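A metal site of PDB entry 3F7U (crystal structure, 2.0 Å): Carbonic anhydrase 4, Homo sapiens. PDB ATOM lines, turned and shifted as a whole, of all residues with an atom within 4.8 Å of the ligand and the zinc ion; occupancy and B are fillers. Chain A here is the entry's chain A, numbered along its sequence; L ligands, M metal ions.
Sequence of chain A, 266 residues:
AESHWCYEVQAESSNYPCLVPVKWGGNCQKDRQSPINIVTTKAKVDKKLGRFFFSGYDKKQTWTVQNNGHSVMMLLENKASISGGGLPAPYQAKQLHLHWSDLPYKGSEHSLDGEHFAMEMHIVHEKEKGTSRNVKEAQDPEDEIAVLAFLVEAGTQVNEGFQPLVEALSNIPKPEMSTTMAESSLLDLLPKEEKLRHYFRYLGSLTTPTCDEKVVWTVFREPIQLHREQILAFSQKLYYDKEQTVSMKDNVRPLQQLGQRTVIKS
The backbone NH (N) of Thr 207 sits at hydrogen-bond distance from an oxygen (O4) of the ligand (3.0 Å).
N3 of the ligand lies close to OG1 of Thr 207 (2.7 Å).
A nitrogen (N1) of the ligand is in hydrogen-bond range of the side-chain hydroxyl (OG1) of Thr 208, 2.8 Å away.
The side-chain amide nitrogen (NE2) of Gln 95 sits at hydrogen-bond distance from an oxygen (O1) of the ligand (2.9 Å).
A ring nitrogen (ND1) of His 97 is in hydrogen-bond range of the side-chain amide oxygen (OE1) of Gln 95 (2.8 Å).
The side-chain carboxylate of Glu 109 sits close to a ring nitrogen (ND1) of His 99 (3.5 Å).
OG1 of Thr 207 is in hydrogen-bond range of OE1 of Glu 109 (2.5 Å).
The backbone NH (N) of Val 124 is in hydrogen-bond range of the backbone carbonyl oxygen (O) of Gln 95, at 2.9 Å.
The side-chain amide oxygen of Asn 68 lies within hydrogen-bond range of the backbone NH of Ser 71.
N of His 70 is in hydrogen-bond range of OD1 of Asn 68, 2.8 Å away.
The backbone NH (N) of Lys 94 is in hydrogen-bond range of the backbone carbonyl oxygen (O) of Val 124.
The backbone carbonyl oxygen of Ser 205 lies within hydrogen-bond range of the indole nitrogen of Trp 217 (2.8 Å).
Residues that only touch the ligand: Leu 206, Asn 68, Ser 71, Val 124, Trp 217, His 70, Val 147 and Glu 126.
Hydrophobic or aromatic side chains within 4 Å of the ligand: His 70, His 97, His 99, His 122, Val 124, Val 147, Leu 206 and Trp 217.
14 residues have an atom within 4 Å of the ligand: Asn 68, His 70, Ser 71, Gln 95, His 97, His 99, His 122, Val 124, Glu 126, Val 147, Leu 206, Thr 207, Thr 208 and Trp 217.
Thr 207 touches the zinc ion (OG1 to ZN, 3.9 Å).
Within 4 Å of the zinc ion: His 97, His 99, His 122 and Thr 207.
The nearest printed residue that does not touch the zinc ion is Glu 109 (4.1 Å).
NE2 of His 97 binds the zinc ion (1.9 Å).
The zinc ion is bound by a ring nitrogen (ND1) of His 122 (1.9 Å).
The zinc ion is bound by N3 of the ligand (2.0 Å).
NE2 of His 99 binds the zinc ion (2.0 Å).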
ATOM      1  N   TRP A   5      12.922   5.563  29.653  1.00  0.00           N
ATOM      2  CA  TRP A   5      12.861   6.343  28.371  1.00  0.00           C
ATOM      3  C   TRP A   5      13.111   5.430  27.180  1.00  0.00           C
ATOM      4  O   TRP A   5      13.632   4.338  27.332  1.00  0.00           O
ATOM      5  CB  TRP A   5      13.818   7.566  28.353  1.00  0.00           C
ATOM      6  CG  TRP A   5      15.279   7.226  28.234  1.00  0.00           C
ATOM      7  CD1 TRP A   5      16.148   6.995  29.232  1.00  0.00           C
ATOM      8  CD2 TRP A   5      16.012   7.062  26.998  1.00  0.00           C
ATOM      9  NE1 TRP A   5      17.423   6.720  28.704  1.00  0.00           N
ATOM     10  CE2 TRP A   5      17.344   6.770  27.332  1.00  0.00           C
ATOM     11  CE3 TRP A   5      15.668   7.201  25.656  1.00  0.00           C
ATOM     12  CZ2 TRP A   5      18.351   6.574  26.363  1.00  0.00           C
ATOM     13  CZ3 TRP A   5      16.653   6.969  24.687  1.00  0.00           C
ATOM     14  CH2 TRP A   5      17.981   6.673  25.070  1.00  0.00           C
ATOM     15  N   TYR A   7      13.025   5.263  22.471  1.00  0.00           N
ATOM     16  CA  TYR A   7      12.706   5.838  21.193  1.00  0.00           C
ATOM     17  C   TYR A   7      11.276   5.472  20.642  1.00  0.00           C
ATOM     18  O   TYR A   7      10.706   4.402  20.965  1.00  0.00           O
ATOM     19  CB  TYR A   7      13.816   5.447  20.218  1.00  0.00           C
ATOM     20  CG  TYR A   7      15.197   6.026  20.574  1.00  0.00           C
ATOM     21  CD1 TYR A   7      15.483   7.366  20.319  1.00  0.00           C
ATOM     22  CD2 TYR A   7      16.200   5.214  21.113  1.00  0.00           C
ATOM     23  CE1 TYR A   7      16.710   7.917  20.631  1.00  0.00           C
ATOM     24  CE2 TYR A   7      17.413   5.727  21.461  1.00  0.00           C
ATOM     25  CZ  TYR A   7      17.682   7.109  21.152  1.00  0.00           C
ATOM     26  OH  TYR A   7      18.891   7.617  21.443  1.00  0.00           O
ATOM     27  N   ASN A  68      24.187  -1.231  24.992  1.00  0.00           N
ATOM     28  CA  ASN A  68      23.667  -0.672  26.287  1.00  0.00           C
ATOM     29  C   ASN A  68      22.167  -0.548  26.214  1.00  0.00           C
ATOM     30  O   ASN A  68      21.513   0.100  27.033  1.00  0.00           O
ATOM     31  CB  ASN A  68      24.327   0.663  26.679  1.00  0.00           C
ATOM     32  CG  ASN A  68      23.942   1.805  25.734  1.00  0.00           C
ATOM     33  OD1 ASN A  68      23.241   1.583  24.764  1.00  0.00           O
ATOM     34  ND2 ASN A  68      24.376   3.046  26.035  1.00  0.00           N
ATOM     35  N   HIS A  70      20.558   1.123  24.016  1.00  0.00           N
ATOM     36  CA  HIS A  70      20.086   2.288  23.260  1.00  0.00           C
ATOM     37  C   HIS A  70      20.918   2.432  21.983  1.00  0.00           C
ATOM     38  O   HIS A  70      20.555   3.138  21.021  1.00  0.00           O
ATOM     39  CB  HIS A  70      20.203   3.594  24.093  1.00  0.00           C
ATOM     40  CG  HIS A  70      19.572   3.480  25.461  1.00  0.00           C
ATOM     41  ND1 HIS A  70      18.207   3.395  25.629  1.00  0.00           N
ATOM     42  CD2 HIS A  70      20.108   3.471  26.718  1.00  0.00           C
ATOM     43  CE1 HIS A  70      17.920   3.347  26.918  1.00  0.00           C
ATOM     44  NE2 HIS A  70      19.055   3.357  27.612  1.00  0.00           N
ATOM     45  N   SER A  71      22.078   1.800  22.010  1.00  0.00           N
ATOM     46  CA  SER A  71      23.022   1.965  20.922  1.00  0.00           C
ATOM     47  C   SER A  71      24.086   0.952  21.151  1.00  0.00           C
ATOM     48  O   SER A  71      23.948   0.121  22.057  1.00  0.00           O
ATOM     49  CB  SER A  71      23.597   3.390  20.980  1.00  0.00           C
ATOM     50  OG  SER A  71      24.539   3.539  19.957  1.00  0.00           O
ATOM     51  N   LYS A  94      35.688  10.159  25.778  1.00  0.00           N
ATOM     52  CA  LYS A  94      35.086   9.214  26.739  1.00  0.00           C
ATOM     53  C   LYS A  94      34.444   7.968  26.130  1.00  0.00           C
ATOM     54  O   LYS A  94      34.518   6.853  26.676  1.00  0.00           O
ATOM     55  CB  LYS A  94      34.006   9.943  27.563  1.00  0.00           C
ATOM     56  CG  LYS A  94      34.469  11.191  28.302  1.00  0.00           C
ATOM     57  CD  LYS A  94      35.287  10.859  29.564  1.00  0.00           C
ATOM     58  CE  LYS A  94      35.992  12.129  30.093  1.00  0.00           C
ATOM     59  NZ  LYS A  94      37.127  11.914  31.085  1.00  0.00           N
ATOM     60  N   GLN A  95      33.677   8.166  25.037  1.00  0.00           N
ATOM     61  CA  GLN A  95      32.973   7.073  24.435  1.00  0.00           C
ATOM     62  C   GLN A  95      32.554   7.481  23.027  1.00  0.00           C
ATOM     63  O   GLN A  95      32.414   8.673  22.741  1.00  0.00           O
ATOM     64  CB  GLN A  95      31.790   6.569  25.265  1.00  0.00           C
ATOM     65  CG  GLN A  95      30.814   7.668  25.718  1.00  0.00           C
ATOM     66  CD  GLN A  95      29.409   7.540  25.128  1.00  0.00           C
ATOM     67  OE1 GLN A  95      29.218   7.320  23.936  1.00  0.00           O
ATOM     68  NE2 GLN A  95      28.403   7.698  25.985  1.00  0.00           N
ATOM     69  N   HIS A  97      29.586   6.330  20.105  1.00  0.00           N
ATOM     70  CA  HIS A  97      28.408   5.484  19.865  1.00  0.00           C
ATOM     71  C   HIS A  97      27.784   5.939  18.524  1.00  0.00           C
ATOM     72  O   HIS A  97      28.282   6.879  17.902  1.00  0.00           O
ATOM     73  CB  HIS A  97      27.381   5.573  21.022  1.00  0.00           C
ATOM     74  CG  HIS A  97      26.790   6.936  21.175  1.00  0.00           C
ATOM     75  ND1 HIS A  97      27.387   7.904  21.936  1.00  0.00           N
ATOM     76  CD2 HIS A  97      25.767   7.551  20.523  1.00  0.00           C
ATOM     77  CE1 HIS A  97      26.703   9.040  21.842  1.00  0.00           C
ATOM     78  NE2 HIS A  97      25.723   8.864  20.960  1.00  0.00           N
ATOM     79  N   HIS A  99      23.950   6.301  15.931  1.00  0.00           N
ATOM     80  CA  HIS A  99      22.510   6.352  15.762  1.00  0.00           C
ATOM     81  C   HIS A  99      22.277   5.916  14.300  1.00  0.00           C
ATOM     82  O   HIS A  99      23.017   6.304  13.427  1.00  0.00           O
ATOM     83  CB  HIS A  99      21.995   7.829  16.003  1.00  0.00           C
ATOM     84  CG  HIS A  99      22.300   8.379  17.382  1.00  0.00           C
ATOM     85  ND1 HIS A  99      21.396   8.309  18.441  1.00  0.00           N
ATOM     86  CD2 HIS A  99      23.403   8.973  17.892  1.00  0.00           C
ATOM     87  CE1 HIS A  99      21.959   8.806  19.544  1.00  0.00           C
ATOM     88  NE2 HIS A  99      23.183   9.203  19.237  1.00  0.00           N
ATOM     89  N   GLU A 109      21.057  11.976  13.346  1.00  0.00           N
ATOM     90  CA  GLU A 109      20.271  12.829  14.225  1.00  0.00           C
ATOM     91  C   GLU A 109      20.144  14.272  13.648  1.00  0.00           C
ATOM     92  O   GLU A 109      19.063  14.836  13.527  1.00  0.00           O
ATOM     93  CB  GLU A 109      20.834  12.812  15.656  1.00  0.00           C
ATOM     94  CG  GLU A 109      20.825  11.347  16.297  1.00  0.00           C
ATOM     95  CD  GLU A 109      20.501  11.457  17.751  1.00  0.00           C
ATOM     96  OE1 GLU A 109      21.366  11.903  18.442  1.00  0.00           O
ATOM     97  OE2 GLU A 109      19.381  11.122  18.216  1.00  0.00           O
ATOM     98  N   HIS A 122      28.755   9.697  17.060  1.00  0.00           N
ATOM     99  CA  HIS A 122      29.079  10.716  18.031  1.00  0.00           C
ATOM    100  C   HIS A 122      30.255  10.285  18.861  1.00  0.00           C
ATOM    101  O   HIS A 122      30.177   9.205  19.495  1.00  0.00           O
ATOM    102  CB  HIS A 122      27.916  10.842  18.986  1.00  0.00           C
ATOM    103  CG  HIS A 122      26.698  11.470  18.383  1.00  0.00           C
ATOM    104  ND1 HIS A 122      25.442  11.312  18.923  1.00  0.00           N
ATOM    105  CD2 HIS A 122      26.546  12.255  17.277  1.00  0.00           C
ATOM    106  CE1 HIS A 122      24.565  11.963  18.164  1.00  0.00           C
ATOM    107  NE2 HIS A 122      25.215  12.574  17.177  1.00  0.00           N
ATOM    108  N   VAL A 124      32.076  11.436  22.048  1.00  0.00           N
ATOM    109  CA  VAL A 124      31.753  12.296  23.177  1.00  0.00           C
ATOM    110  C   VAL A 124      33.015  12.573  23.978  1.00  0.00           C
ATOM    111  O   VAL A 124      33.718  11.632  24.420  1.00  0.00           O
ATOM    112  CB  VAL A 124      30.786  11.549  24.037  1.00  0.00           C
ATOM    113  CG1 VAL A 124      30.372  12.401  25.263  1.00  0.00           C
ATOM    114  CG2 VAL A 124      29.544  11.165  23.209  1.00  0.00           C
ATOM    115  N   GLU A 126      35.055  15.331  26.988  1.00  0.00           N
ATOM    116  CA  GLU A 126      34.742  16.180  28.133  1.00  0.00           C
ATOM    117  C   GLU A 126      35.896  17.136  28.430  1.00  0.00           C
ATOM    118  O   GLU A 126      37.042  16.797  28.232  1.00  0.00           O
ATOM    119  CB  GLU A 126      34.428  15.283  29.323  1.00  0.00           C
ATOM    120  CG  GLU A 126      34.476  15.997  30.650  1.00  0.00           C
ATOM    121  CD  GLU A 126      33.219  15.695  31.490  1.00  0.00           C
ATOM    122  OE1 GLU A 126      32.615  14.594  31.276  1.00  0.00           O
ATOM    123  OE2 GLU A 126      32.855  16.572  32.336  1.00  0.00           O
ATOM    124  N   ILE A 145      30.899  19.566  27.534  1.00  0.00           N
ATOM    125  CA  ILE A 145      30.985  18.380  26.646  1.00  0.00           C
ATOM    126  C   ILE A 145      31.102  18.793  25.162  1.00  0.00           C
ATOM    127  O   ILE A 145      30.307  19.657  24.693  1.00  0.00           O
ATOM    128  CB  ILE A 145      29.726  17.440  26.864  1.00  0.00           C
ATOM    129  CG1 ILE A 145      29.848  16.756  28.219  1.00  0.00           C
ATOM    130  CG2 ILE A 145      29.756  16.275  25.948  1.00  0.00           C
ATOM    131  CD1 ILE A 145      29.163  17.455  29.231  1.00  0.00           C
ATOM    132  N   VAL A 147      30.941  17.161  21.563  1.00  0.00           N
ATOM    133  CA  VAL A 147      30.623  15.957  20.817  1.00  0.00           C
ATOM    134  C   VAL A 147      31.012  16.199  19.351  1.00  0.00           C
ATOM    135  O   VAL A 147      30.704  17.266  18.767  1.00  0.00           O
ATOM    136  CB  VAL A 147      29.150  15.621  20.851  1.00  0.00           C
ATOM    137  CG1 VAL A 147      28.922  14.406  19.951  1.00  0.00           C
ATOM    138  CG2 VAL A 147      28.753  15.333  22.319  1.00  0.00           C
ATOM    139  N   SER A 205      22.469  20.277  23.304  1.00  0.00           N
ATOM    140  CA  SER A 205      22.161  19.382  24.416  1.00  0.00           C
ATOM    141  C   SER A 205      22.656  18.023  24.066  1.00  0.00           C
ATOM    142  O   SER A 205      23.010  17.769  22.908  1.00  0.00           O
ATOM    143  CB  SER A 205      20.652  19.341  24.679  1.00  0.00           C
ATOM    144  OG  SER A 205      19.943  18.622  23.642  1.00  0.00           O
ATOM    145  N   LEU A 206      22.678  17.137  25.064  1.00  0.00           N
ATOM    146  CA  LEU A 206      22.777  15.719  24.781  1.00  0.00           C
ATOM    147  C   LEU A 206      21.446  15.345  24.092  1.00  0.00           C
ATOM    148  O   LEU A 206      20.410  15.971  24.414  1.00  0.00           O
ATOM    149  CB  LEU A 206      22.813  14.980  26.101  1.00  0.00           C
ATOM    150  CG  LEU A 206      24.015  15.331  27.012  1.00  0.00           C
ATOM    151  CD1 LEU A 206      23.852  14.477  28.337  1.00  0.00           C
ATOM    152  CD2 LEU A 206      25.300  14.970  26.290  1.00  0.00           C
ATOM    153  N   THR A 207      21.458  14.305  23.245  1.00  0.00           N
ATOM    154  CA  THR A 207      20.246  13.897  22.485  1.00  0.00           C
ATOM    155  C   THR A 207      19.515  12.719  23.160  1.00  0.00           C
ATOM    156  O   THR A 207      18.593  12.130  22.591  1.00  0.00           O
ATOM    157  CB  THR A 207      20.565  13.547  20.986  1.00  0.00           C
ATOM    158  OG1 THR A 207      21.400  12.371  20.921  1.00  0.00           O
ATOM    159  CG2 THR A 207      21.283  14.694  20.327  1.00  0.00           C
ATOM    160  N   THR A 208      19.909  12.387  24.396  1.00  0.00           N
ATOM    161  CA  THR A 208      19.182  11.345  25.199  1.00  0.00           C
ATOM    162  C   THR A 208      19.059  11.897  26.595  1.00  0.00           C
ATOM    163  O   THR A 208      19.900  12.706  26.978  1.00  0.00           O
ATOM    164  CB  THR A 208      20.015   9.999  25.292  1.00  0.00           C
ATOM    165  OG1 THR A 208      21.309  10.279  25.855  1.00  0.00           O
ATOM    166  CG2 THR A 208      20.239   9.413  23.803  1.00  0.00           C
ATOM    167  N   LYS A 214      24.622  21.181  27.717  1.00  0.00           N
ATOM    168  CA  LYS A 214      26.029  21.367  28.026  1.00  0.00           C
ATOM    169  C   LYS A 214      27.008  21.000  26.942  1.00  0.00           C
ATOM    170  O   LYS A 214      28.220  20.833  27.213  1.00  0.00           O
ATOM    171  CB  LYS A 214      26.384  20.580  29.290  1.00  0.00           C
ATOM    172  CG  LYS A 214      26.019  19.069  29.225  1.00  0.00           C
ATOM    173  CD  LYS A 214      26.371  18.428  30.666  1.00  0.00           C
ATOM    174  CE  LYS A 214      26.263  16.857  30.675  1.00  0.00           C
ATOM    175  NZ  LYS A 214      26.504  16.109  32.053  1.00  0.00           N
ATOM    176  N   TRP A 217      28.642  21.350  19.986  1.00  0.00           N
ATOM    177  CA  TRP A 217      28.394  20.356  18.908  1.00  0.00           C
ATOM    178  C   TRP A 217      29.321  20.719  17.780  1.00  0.00           C
ATOM    179  O   TRP A 217      29.569  21.913  17.550  1.00  0.00           O
ATOM    180  CB  TRP A 217      26.885  20.417  18.454  1.00  0.00           C
ATOM    181  CG  TRP A 217      26.037  19.471  19.274  1.00  0.00           C
ATOM    182  CD1 TRP A 217      25.266  19.796  20.361  1.00  0.00           C
ATOM    183  CD2 TRP A 217      25.958  18.048  19.128  1.00  0.00           C
ATOM    184  NE1 TRP A 217      24.671  18.669  20.877  1.00  0.00           N
ATOM    185  CE2 TRP A 217      25.061  17.579  20.124  1.00  0.00           C
ATOM    186  CE3 TRP A 217      26.521  17.138  18.242  1.00  0.00           C
ATOM    187  CZ2 TRP A 217      24.784  16.198  20.303  1.00  0.00           C
ATOM    188  CZ3 TRP A 217      26.195  15.762  18.366  1.00  0.00           C
ATOM    189  CH2 TRP A 217      25.343  15.314  19.387  1.00  0.00           C
HETATM  190  O1  LIG L   1      25.500   7.773  26.274  1.00  0.00           O
HETATM  191  C1  LIG L   1      24.687   8.672  26.114  1.00  0.00           C
HETATM  192  N1  LIG L   1      23.378   8.487  26.308  1.00  0.00           N
HETATM  193  C2  LIG L   1      23.038   7.291  27.062  1.00  0.00           C
HETATM  194  C3  LIG L   1      22.860   6.063  26.211  1.00  0.00           C
HETATM  195  C4  LIG L   1      22.341   6.410  24.831  1.00  0.00           C
HETATM  196  O2  LIG L   1      23.242   5.809  23.901  1.00  0.00           O
HETATM  197  C5  LIG L   1      23.012   6.468  22.658  1.00  0.00           C
HETATM  198  C6  LIG L   1      25.267   9.934  25.597  1.00  0.00           C
HETATM  199  C7  LIG L   1      24.776  10.421  24.398  1.00  0.00           C
HETATM  200  C8  LIG L   1      26.280  10.547  26.345  1.00  0.00           C
HETATM  201  N2  LIG L   1      26.810  11.648  25.816  1.00  0.00           N
HETATM  202  C9  LIG L   1      26.387  12.153  24.624  1.00  0.00           C
HETATM  203  C10 LIG L   1      25.377  11.564  23.882  1.00  0.00           C
HETATM  204  S1  LIG L   1      24.942  12.237  22.466  1.00  0.00           S
HETATM  205  O3  LIG L   1      26.214  12.392  21.657  1.00  0.00           O
HETATM  206  O4  LIG L   1      24.292  13.611  22.768  1.00  0.00           O
HETATM  207  N3  LIG L   1      23.763  11.355  21.799  1.00  0.00           N
HETATM  208  S2  LIG L   1      26.789   9.872  27.869  1.00  0.00           S
HETATM  209  C11 LIG L   1      28.052  10.881  28.396  1.00  0.00           C
HETATM  210  C12 LIG L   1      27.760  12.177  28.863  1.00  0.00           C
HETATM  211  C13 LIG L   1      28.824  12.983  29.307  1.00  0.00           C
HETATM  212  C14 LIG L   1      30.125  12.501  29.299  1.00  0.00           C
HETATM  213  C15 LIG L   1      30.428  11.194  28.847  1.00  0.00           C
HETATM  214  C16 LIG L   1      29.373  10.398  28.396  1.00  0.00           C
HETATM  215 ZN    ZN M   1      24.568  10.258  20.302  1.00  0.00          ZN
